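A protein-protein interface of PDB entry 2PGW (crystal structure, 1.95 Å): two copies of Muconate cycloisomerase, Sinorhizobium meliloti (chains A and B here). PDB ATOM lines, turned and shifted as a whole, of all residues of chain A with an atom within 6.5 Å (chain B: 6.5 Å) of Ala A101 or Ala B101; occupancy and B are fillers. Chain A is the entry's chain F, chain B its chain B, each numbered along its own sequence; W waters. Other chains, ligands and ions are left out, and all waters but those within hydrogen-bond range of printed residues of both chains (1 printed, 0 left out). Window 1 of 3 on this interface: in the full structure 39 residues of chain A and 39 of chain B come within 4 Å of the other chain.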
ATOM      1  N   TYR A  91      21.394 -35.959  -6.968  1.00  0.00           N
ATOM      2  CA  TYR A  91      22.750 -35.463  -7.186  1.00  0.00           C
ATOM      3  C   TYR A  91      23.713 -35.784  -6.045  1.00  0.00           C
ATOM      4  O   TYR A  91      24.634 -36.583  -6.198  1.00  0.00           O
ATOM      5  CB  TYR A  91      22.729 -33.943  -7.391  1.00  0.00           C
ATOM      6  CG  TYR A  91      22.119 -33.459  -8.688  1.00  0.00           C
ATOM      7  CD1 TYR A  91      22.922 -33.184  -9.803  1.00  0.00           C
ATOM      8  CD2 TYR A  91      20.749 -33.214  -8.784  1.00  0.00           C
ATOM      9  CE1 TYR A  91      22.366 -32.668 -10.978  1.00  0.00           C
ATOM     10  CE2 TYR A  91      20.185 -32.701  -9.952  1.00  0.00           C
ATOM     11  CZ  TYR A  91      20.997 -32.431 -11.039  1.00  0.00           C
ATOM     12  OH  TYR A  91      20.437 -31.921 -12.181  1.00  0.00           O
ATOM     13  N   ILE A  98      27.333 -31.045  -8.103  1.00  0.00           N
ATOM     14  CA  ILE A  98      27.360 -30.089  -9.192  1.00  0.00           C
ATOM     15  C   ILE A  98      26.194 -29.108  -9.069  1.00  0.00           C
ATOM     16  O   ILE A  98      25.207 -29.184  -9.811  1.00  0.00           O
ATOM     17  CB  ILE A  98      27.337 -30.829 -10.551  1.00  0.00           C
ATOM     18  CG1 ILE A  98      26.178 -31.834 -10.585  1.00  0.00           C
ATOM     19  CG2 ILE A  98      28.657 -31.588 -10.751  1.00  0.00           C
ATOM     20  CD1 ILE A  98      26.086 -32.644 -11.882  1.00  0.00           C
ATOM     21  N   MET A  99      26.329 -28.186  -8.118  1.00  0.00           N
ATOM     22  CA  MET A  99      25.294 -27.188  -7.858  1.00  0.00           C
ATOM     23  C   MET A  99      24.920 -26.306  -9.056  1.00  0.00           C
ATOM     24  O   MET A  99      23.739 -26.072  -9.310  1.00  0.00           O
ATOM     25  CB  MET A  99      25.706 -26.300  -6.690  1.00  0.00           C
ATOM     26  CG  MET A  99      24.673 -25.215  -6.343  1.00  0.00           C
ATOM     27  SD  MET A  99      25.017 -24.447  -4.614  1.00  0.00           S
ATOM     28  CE  MET A  99      24.291 -25.816  -3.439  1.00  0.00           C
ATOM     29  N   ARG A 100      25.914 -25.810  -9.782  1.00  0.00           N
ATOM     30  CA  ARG A 100      25.625 -24.965 -10.933  1.00  0.00           C
ATOM     31  C   ARG A 100      24.815 -25.726 -11.987  1.00  0.00           C
ATOM     32  O   ARG A 100      23.878 -25.175 -12.570  1.00  0.00           O
ATOM     33  CB  ARG A 100      26.928 -24.443 -11.545  1.00  0.00           C
ATOM     34  CG  ARG A 100      27.688 -23.458 -10.664  1.00  0.00           C
ATOM     35  CD  ARG A 100      28.878 -22.888 -11.412  1.00  0.00           C
ATOM     36  NE  ARG A 100      29.560 -21.843 -10.661  1.00  0.00           N
ATOM     37  CZ  ARG A 100      30.489 -21.050 -11.175  1.00  0.00           C
ATOM     38  NH1 ARG A 100      30.840 -21.193 -12.447  1.00  0.00           N
ATOM     39  NH2 ARG A 100      31.062 -20.117 -10.422  1.00  0.00           N
ATOM     40  N   ALA A 101      25.173 -26.986 -12.218  1.00  0.00           N
ATOM     41  CA  ALA A 101      24.471 -27.814 -13.202  1.00  0.00           C
ATOM     42  C   ALA A 101      23.031 -28.061 -12.769  1.00  0.00           C
ATOM     43  O   ALA A 101      22.112 -27.964 -13.573  1.00  0.00           O
ATOM     44  CB  ALA A 101      25.193 -29.139 -13.396  1.00  0.00           C
ATOM     45  N   ALA A 102      22.837 -28.374 -11.489  1.00  0.00           N
ATOM     46  CA  ALA A 102      21.490 -28.618 -10.984  1.00  0.00           C
ATOM     47  C   ALA A 102      20.628 -27.347 -11.020  1.00  0.00           C
ATOM     48  O   ALA A 102      19.427 -27.415 -11.310  1.00  0.00           O
ATOM     49  CB  ALA A 102      21.562 -29.166  -9.566  1.00  0.00           C
ATOM     50  N   ASN A 103      21.243 -26.198 -10.744  1.00  0.00           N
ATOM     51  CA  ASN A 103      20.544 -24.914 -10.748  1.00  0.00           C
ATOM     52  C   ASN A 103      19.937 -24.670 -12.127  1.00  0.00           C
ATOM     53  O   ASN A 103      18.834 -24.133 -12.252  1.00  0.00           O
ATOM     54  CB  ASN A 103      21.519 -23.768 -10.415  1.00  0.00           C
ATOM     55  CG  ASN A 103      21.837 -23.668  -8.922  1.00  0.00           C
ATOM     56  OD1 ASN A 103      21.345 -24.446  -8.113  1.00  0.00           O
ATOM     57  ND2 ASN A 103      22.668 -22.697  -8.562  1.00  0.00           N
ATOM     58  N   GLN A 104      20.685 -25.059 -13.157  1.00  0.00           N
ATOM     59  CA  GLN A 104      20.270 -24.895 -14.548  1.00  0.00           C
ATOM     60  C   GLN A 104      18.920 -25.557 -14.797  1.00  0.00           C
ATOM     61  O   GLN A 104      18.069 -25.018 -15.501  1.00  0.00           O
ATOM     62  CB  GLN A 104      21.316 -25.524 -15.470  1.00  0.00           C
ATOM     63  CG  GLN A 104      21.073 -25.267 -16.945  1.00  0.00           C
ATOM     64  CD  GLN A 104      22.032 -26.037 -17.838  1.00  0.00           C
ATOM     65  OE1 GLN A 104      23.219 -26.161 -17.533  1.00  0.00           O
ATOM     66  NE2 GLN A 104      21.521 -26.544 -18.955  1.00  0.00           N
ATOM     67  N   ILE A 105      18.745 -26.738 -14.210  1.00  0.00           N
ATOM     68  CA  ILE A 105      17.522 -27.508 -14.348  1.00  0.00           C
ATOM     69  C   ILE A 105      16.437 -27.007 -13.390  1.00  0.00           C
ATOM     70  O   ILE A 105      15.306 -26.753 -13.807  1.00  0.00           O
ATOM     71  CB  ILE A 105      17.793 -29.003 -14.082  1.00  0.00           C
ATOM     72  CG1 ILE A 105      18.950 -29.478 -14.963  1.00  0.00           C
ATOM     73  CG2 ILE A 105      16.540 -29.823 -14.361  1.00  0.00           C
ATOM     74  CD1 ILE A 105      18.749 -29.217 -16.449  1.00  0.00           C
ATOM     75  N   PHE A 106      16.782 -26.855 -12.117  1.00  0.00           N
ATOM     76  CA  PHE A 106      15.813 -26.376 -11.139  1.00  0.00           C
ATOM     77  C   PHE A 106      15.301 -24.978 -11.461  1.00  0.00           C
ATOM     78  O   PHE A 106      14.230 -24.593 -10.993  1.00  0.00           O
ATOM     79  CB  PHE A 106      16.407 -26.404  -9.728  1.00  0.00           C
ATOM     80  CG  PHE A 106      16.587 -27.782  -9.178  1.00  0.00           C
ATOM     81  CD1 PHE A 106      15.502 -28.659  -9.083  1.00  0.00           C
ATOM     82  CD2 PHE A 106      17.839 -28.220  -8.760  1.00  0.00           C
ATOM     83  CE1 PHE A 106      15.665 -29.955  -8.578  1.00  0.00           C
ATOM     84  CE2 PHE A 106      18.018 -29.511  -8.250  1.00  0.00           C
ATOM     85  CZ  PHE A 106      16.927 -30.380  -8.158  1.00  0.00           C
ATOM     86  N   PHE A 251      27.343 -17.690  -9.839  1.00  0.00           N
ATOM     87  CA  PHE A 251      26.273 -18.617 -10.211  1.00  0.00           C
ATOM     88  C   PHE A 251      25.458 -19.031  -8.996  1.00  0.00           C
ATOM     89  O   PHE A 251      24.229 -18.972  -9.008  1.00  0.00           O
ATOM     90  CB  PHE A 251      26.842 -19.887 -10.862  1.00  0.00           C
ATOM     91  CG  PHE A 251      26.859 -19.849 -12.370  1.00  0.00           C
ATOM     92  CD1 PHE A 251      27.639 -18.910 -13.048  1.00  0.00           C
ATOM     93  CD2 PHE A 251      26.124 -20.770 -13.116  1.00  0.00           C
ATOM     94  CE1 PHE A 251      27.696 -18.885 -14.450  1.00  0.00           C
ATOM     95  CE2 PHE A 251      26.168 -20.758 -14.524  1.00  0.00           C
ATOM     96  CZ  PHE A 251      26.960 -19.810 -15.190  1.00  0.00           C
ATOM     97  N   TYR B  91      29.849 -25.923 -23.708  1.00  0.00           N
ATOM     98  CA  TYR B  91      29.429 -25.394 -22.415  1.00  0.00           C
ATOM     99  C   TYR B  91      29.511 -23.878 -22.292  1.00  0.00           C
ATOM    100  O   TYR B  91      28.486 -23.196 -22.259  1.00  0.00           O
ATOM    101  CB  TYR B  91      30.269 -26.013 -21.296  1.00  0.00           C
ATOM    102  CG  TYR B  91      30.000 -27.479 -21.028  1.00  0.00           C
ATOM    103  CD1 TYR B  91      29.025 -27.871 -20.107  1.00  0.00           C
ATOM    104  CD2 TYR B  91      30.740 -28.477 -21.672  1.00  0.00           C
ATOM    105  CE1 TYR B  91      28.798 -29.220 -19.828  1.00  0.00           C
ATOM    106  CE2 TYR B  91      30.522 -29.828 -21.397  1.00  0.00           C
ATOM    107  CZ  TYR B  91      29.552 -30.188 -20.473  1.00  0.00           C
ATOM    108  OH  TYR B  91      29.361 -31.517 -20.175  1.00  0.00           O
ATOM    109  N   ILE B  98      29.473 -24.623 -16.006  1.00  0.00           N
ATOM    110  CA  ILE B  98      29.314 -25.663 -15.003  1.00  0.00           C
ATOM    111  C   ILE B  98      30.521 -26.599 -15.055  1.00  0.00           C
ATOM    112  O   ILE B  98      30.437 -27.756 -15.475  1.00  0.00           O
ATOM    113  CB  ILE B  98      27.991 -26.427 -15.243  1.00  0.00           C
ATOM    114  CG1 ILE B  98      27.917 -26.912 -16.701  1.00  0.00           C
ATOM    115  CG2 ILE B  98      26.808 -25.496 -14.953  1.00  0.00           C
ATOM    116  CD1 ILE B  98      26.635 -27.693 -17.043  1.00  0.00           C
ATOM    117  N   MET B  99      31.657 -26.073 -14.621  1.00  0.00           N
ATOM    118  CA  MET B  99      32.904 -26.824 -14.635  1.00  0.00           C
ATOM    119  C   MET B  99      32.843 -28.199 -13.979  1.00  0.00           C
ATOM    120  O   MET B  99      33.289 -29.190 -14.562  1.00  0.00           O
ATOM    121  CB  MET B  99      34.007 -25.987 -13.997  1.00  0.00           C
ATOM    122  CG  MET B  99      35.398 -26.647 -14.045  1.00  0.00           C
ATOM    123  SD  MET B  99      36.788 -25.425 -13.589  1.00  0.00           S
ATOM    124  CE  MET B  99      37.047 -24.485 -15.300  1.00  0.00           C
ATOM    125  N   ARG B 100      32.291 -28.280 -12.771  1.00  0.00           N
ATOM    126  CA  ARG B 100      32.201 -29.559 -12.087  1.00  0.00           C
ATOM    127  C   ARG B 100      31.420 -30.585 -12.909  1.00  0.00           C
ATOM    128  O   ARG B 100      31.852 -31.727 -13.043  1.00  0.00           O
ATOM    129  CB  ARG B 100      31.545 -29.394 -10.725  1.00  0.00           C
ATOM    130  CG  ARG B 100      32.326 -28.517  -9.753  1.00  0.00           C
ATOM    131  CD  ARG B 100      31.690 -28.607  -8.383  1.00  0.00           C
ATOM    132  NE  ARG B 100      32.425 -27.842  -7.384  1.00  0.00           N
ATOM    133  CZ  ARG B 100      32.173 -27.909  -6.085  1.00  0.00           C
ATOM    134  NH1 ARG B 100      31.205 -28.706  -5.644  1.00  0.00           N
ATOM    135  NH2 ARG B 100      32.901 -27.198  -5.228  1.00  0.00           N
ATOM    136  N   ALA B 101      30.276 -30.172 -13.455  1.00  0.00           N
ATOM    137  CA  ALA B 101      29.447 -31.067 -14.259  1.00  0.00           C
ATOM    138  C   ALA B 101      30.221 -31.534 -15.486  1.00  0.00           C
ATOM    139  O   ALA B 101      30.140 -32.702 -15.868  1.00  0.00           O
ATOM    140  CB  ALA B 101      28.165 -30.367 -14.681  1.00  0.00           C
ATOM    141  N   ALA B 102      30.970 -30.628 -16.099  1.00  0.00           N
ATOM    142  CA  ALA B 102      31.776 -30.977 -17.260  1.00  0.00           C
ATOM    143  C   ALA B 102      32.887 -31.961 -16.862  1.00  0.00           C
ATOM    144  O   ALA B 102      33.111 -32.974 -17.538  1.00  0.00           O
ATOM    145  CB  ALA B 102      32.376 -29.710 -17.882  1.00  0.00           C
ATOM    146  N   ASN B 103      33.576 -31.682 -15.756  1.00  0.00           N
ATOM    147  CA  ASN B 103      34.647 -32.572 -15.306  1.00  0.00           C
ATOM    148  C   ASN B 103      34.150 -34.014 -15.195  1.00  0.00           C
ATOM    149  O   ASN B 103      34.870 -34.959 -15.524  1.00  0.00           O
ATOM    150  CB  ASN B 103      35.201 -32.125 -13.949  1.00  0.00           C
ATOM    151  CG  ASN B 103      36.049 -30.871 -14.037  1.00  0.00           C
ATOM    152  OD1 ASN B 103      36.436 -30.435 -15.123  1.00  0.00           O
ATOM    153  ND2 ASN B 103      36.350 -30.289 -12.884  1.00  0.00           N
ATOM    154  N   GLN B 104      32.915 -34.171 -14.726  1.00  0.00           N
ATOM    155  CA  GLN B 104      32.312 -35.493 -14.563  1.00  0.00           C
ATOM    156  C   GLN B 104      32.384 -36.289 -15.859  1.00  0.00           C
ATOM    157  O   GLN B 104      32.657 -37.493 -15.850  1.00  0.00           O
ATOM    158  CB  GLN B 104      30.847 -35.362 -14.146  1.00  0.00           C
ATOM    159  CG  GLN B 104      30.189 -36.675 -13.729  1.00  0.00           C
ATOM    160  CD  GLN B 104      28.712 -36.509 -13.410  1.00  0.00           C
ATOM    161  OE1 GLN B 104      28.293 -35.481 -12.867  1.00  0.00           O
ATOM    162  NE2 GLN B 104      27.916 -37.524 -13.729  1.00  0.00           N
ATOM    163  N   ILE B 105      32.120 -35.618 -16.975  1.00  0.00           N
ATOM    164  CA  ILE B 105      32.129 -36.280 -18.267  1.00  0.00           C
ATOM    165  C   ILE B 105      33.549 -36.391 -18.812  1.00  0.00           C
ATOM    166  O   ILE B 105      33.979 -37.472 -19.221  1.00  0.00           O
ATOM    167  CB  ILE B 105      31.231 -35.535 -19.305  1.00  0.00           C
ATOM    168  CG1 ILE B 105      29.866 -35.196 -18.694  1.00  0.00           C
ATOM    169  CG2 ILE B 105      31.015 -36.416 -20.532  1.00  0.00           C
ATOM    170  CD1 ILE B 105      29.032 -36.398 -18.266  1.00  0.00           C
ATOM    171  N   PHE B 106      34.279 -35.277 -18.805  1.00  0.00           N
ATOM    172  CA  PHE B 106      35.642 -35.266 -19.311  1.00  0.00           C
ATOM    173  C   PHE B 106      36.549 -36.262 -18.605  1.00  0.00           C
ATOM    174  O   PHE B 106      37.534 -36.703 -19.180  1.00  0.00           O
ATOM    175  CB  PHE B 106      36.253 -33.873 -19.213  1.00  0.00           C
ATOM    176  CG  PHE B 106      35.693 -32.892 -20.207  1.00  0.00           C
ATOM    177  CD1 PHE B 106      35.652 -33.198 -21.571  1.00  0.00           C
ATOM    178  CD2 PHE B 106      35.237 -31.645 -19.779  1.00  0.00           C
ATOM    179  CE1 PHE B 106      35.160 -32.267 -22.495  1.00  0.00           C
ATOM    180  CE2 PHE B 106      34.751 -30.715 -20.686  1.00  0.00           C
ATOM    181  CZ  PHE B 106      34.709 -31.019 -22.046  1.00  0.00           C
ATOM    182  N   PHE B 251      36.494 -29.865  -5.887  1.00  0.00           N
ATOM    183  CA  PHE B 251      36.170 -30.511  -7.156  1.00  0.00           C
ATOM    184  C   PHE B 251      37.073 -30.018  -8.292  1.00  0.00           C
ATOM    185  O   PHE B 251      37.681 -30.827  -8.992  1.00  0.00           O
ATOM    186  CB  PHE B 251      34.710 -30.254  -7.557  1.00  0.00           C
ATOM    187  CG  PHE B 251      33.767 -31.358  -7.163  1.00  0.00           C
ATOM    188  CD1 PHE B 251      33.544 -31.673  -5.823  1.00  0.00           C
ATOM    189  CD2 PHE B 251      33.093 -32.083  -8.150  1.00  0.00           C
ATOM    190  CE1 PHE B 251      32.659 -32.698  -5.467  1.00  0.00           C
ATOM    191  CE2 PHE B 251      32.212 -33.103  -7.809  1.00  0.00           C
ATOM    192  CZ  PHE B 251      31.991 -33.416  -6.468  1.00  0.00           C
HETATM  193  O   HOH W   1      28.482 -27.676 -11.949  1.00  0.00           O
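Arg B100 touches Ile A98.
Ala B101 touches Ile A98 (N to CG2, 3.5 Å).
Gln B104 touches Ile A98.
Ile B98 touches Arg A100 (CG2 to CB, 3.6 Å).
N of Ala A101 touches CG2 of Ile B98 (3.5 Å).
CB of Ala B101 touches CB of Ala A101, 3.5 Å away.
Ile B98 touches Gln A104 (CD1 to OE1, 3.8 Å).
Of the printed residues of chain B, Ile A98 touches Arg B100, Ala B101 and Gln B104.
Of the printed residues of chain B, Arg A100 touches Ile B98.
Of chain B, only Ile B98 (3.5 Å) and Ala B101 (3.5 Å) come within 4 Å of Ala A101.
Of the printed residues of chain B, Gln A104 touches Ile B98 (3.8 Å).
Of the printed residues of chain A, Ile B98 touches Arg A100, Ala A101 and Gln A104.
Of the printed residues of chain A, Arg B100 touches Ile A98 (3.6 Å).
Ala B101 touches just these residues of chain A: Ile A98 (3.5 Å) and Ala A101 (3.5 Å).
The nearest residue of chain B that does not touch Ala A101 is Arg B100 (6.4 Å).
The nearest residue of chain A that does not touch Ala B101 is Arg A100 (6.3 Å).
The nearest printed residue of chain A that does not touch Ile B98 is Phe A251 (4.8 Å).
Hydrophobic or aromatic side chains of chain A within 4 Å of the printed part of chain B: Ile A98 and Ala A101.
Printed residues of chain B that touch a printed residue of chain A: Ile B98, Arg B100, Ala B101 and Gln B104.
Hydrophobic or aromatic side chains of chain B that line the printed part of chain A: Ile B98 and Ala B101.
Among the printed residues, 7 pairs touch across the chains.
Among the printed residues, no Asp or Glu carboxylate lies within 4 Å of a Lys or Arg side-chain nitrogen of the other chain.
Ile A98 touches Arg B100, and with the chains exchanged Arg A100 touches Ile B98.
Ile A98 touches Ala B101, and with the chains exchanged Ala A101 touches Ile B98.
Ile A98 touches Gln B104, and with the chains exchanged Gln A104 touches Ile B98.
Ala A101 touches its own counterpart, Ala B101.
Positions printed for both chains: 91, 98, 99, 100, 101, 102, 103, 104, 105, 106 and 251.
Water W1 bridges the backbone NH of Ala A101 (3.4 Å) and the backbone NH of Ala B101 (3.4 Å).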
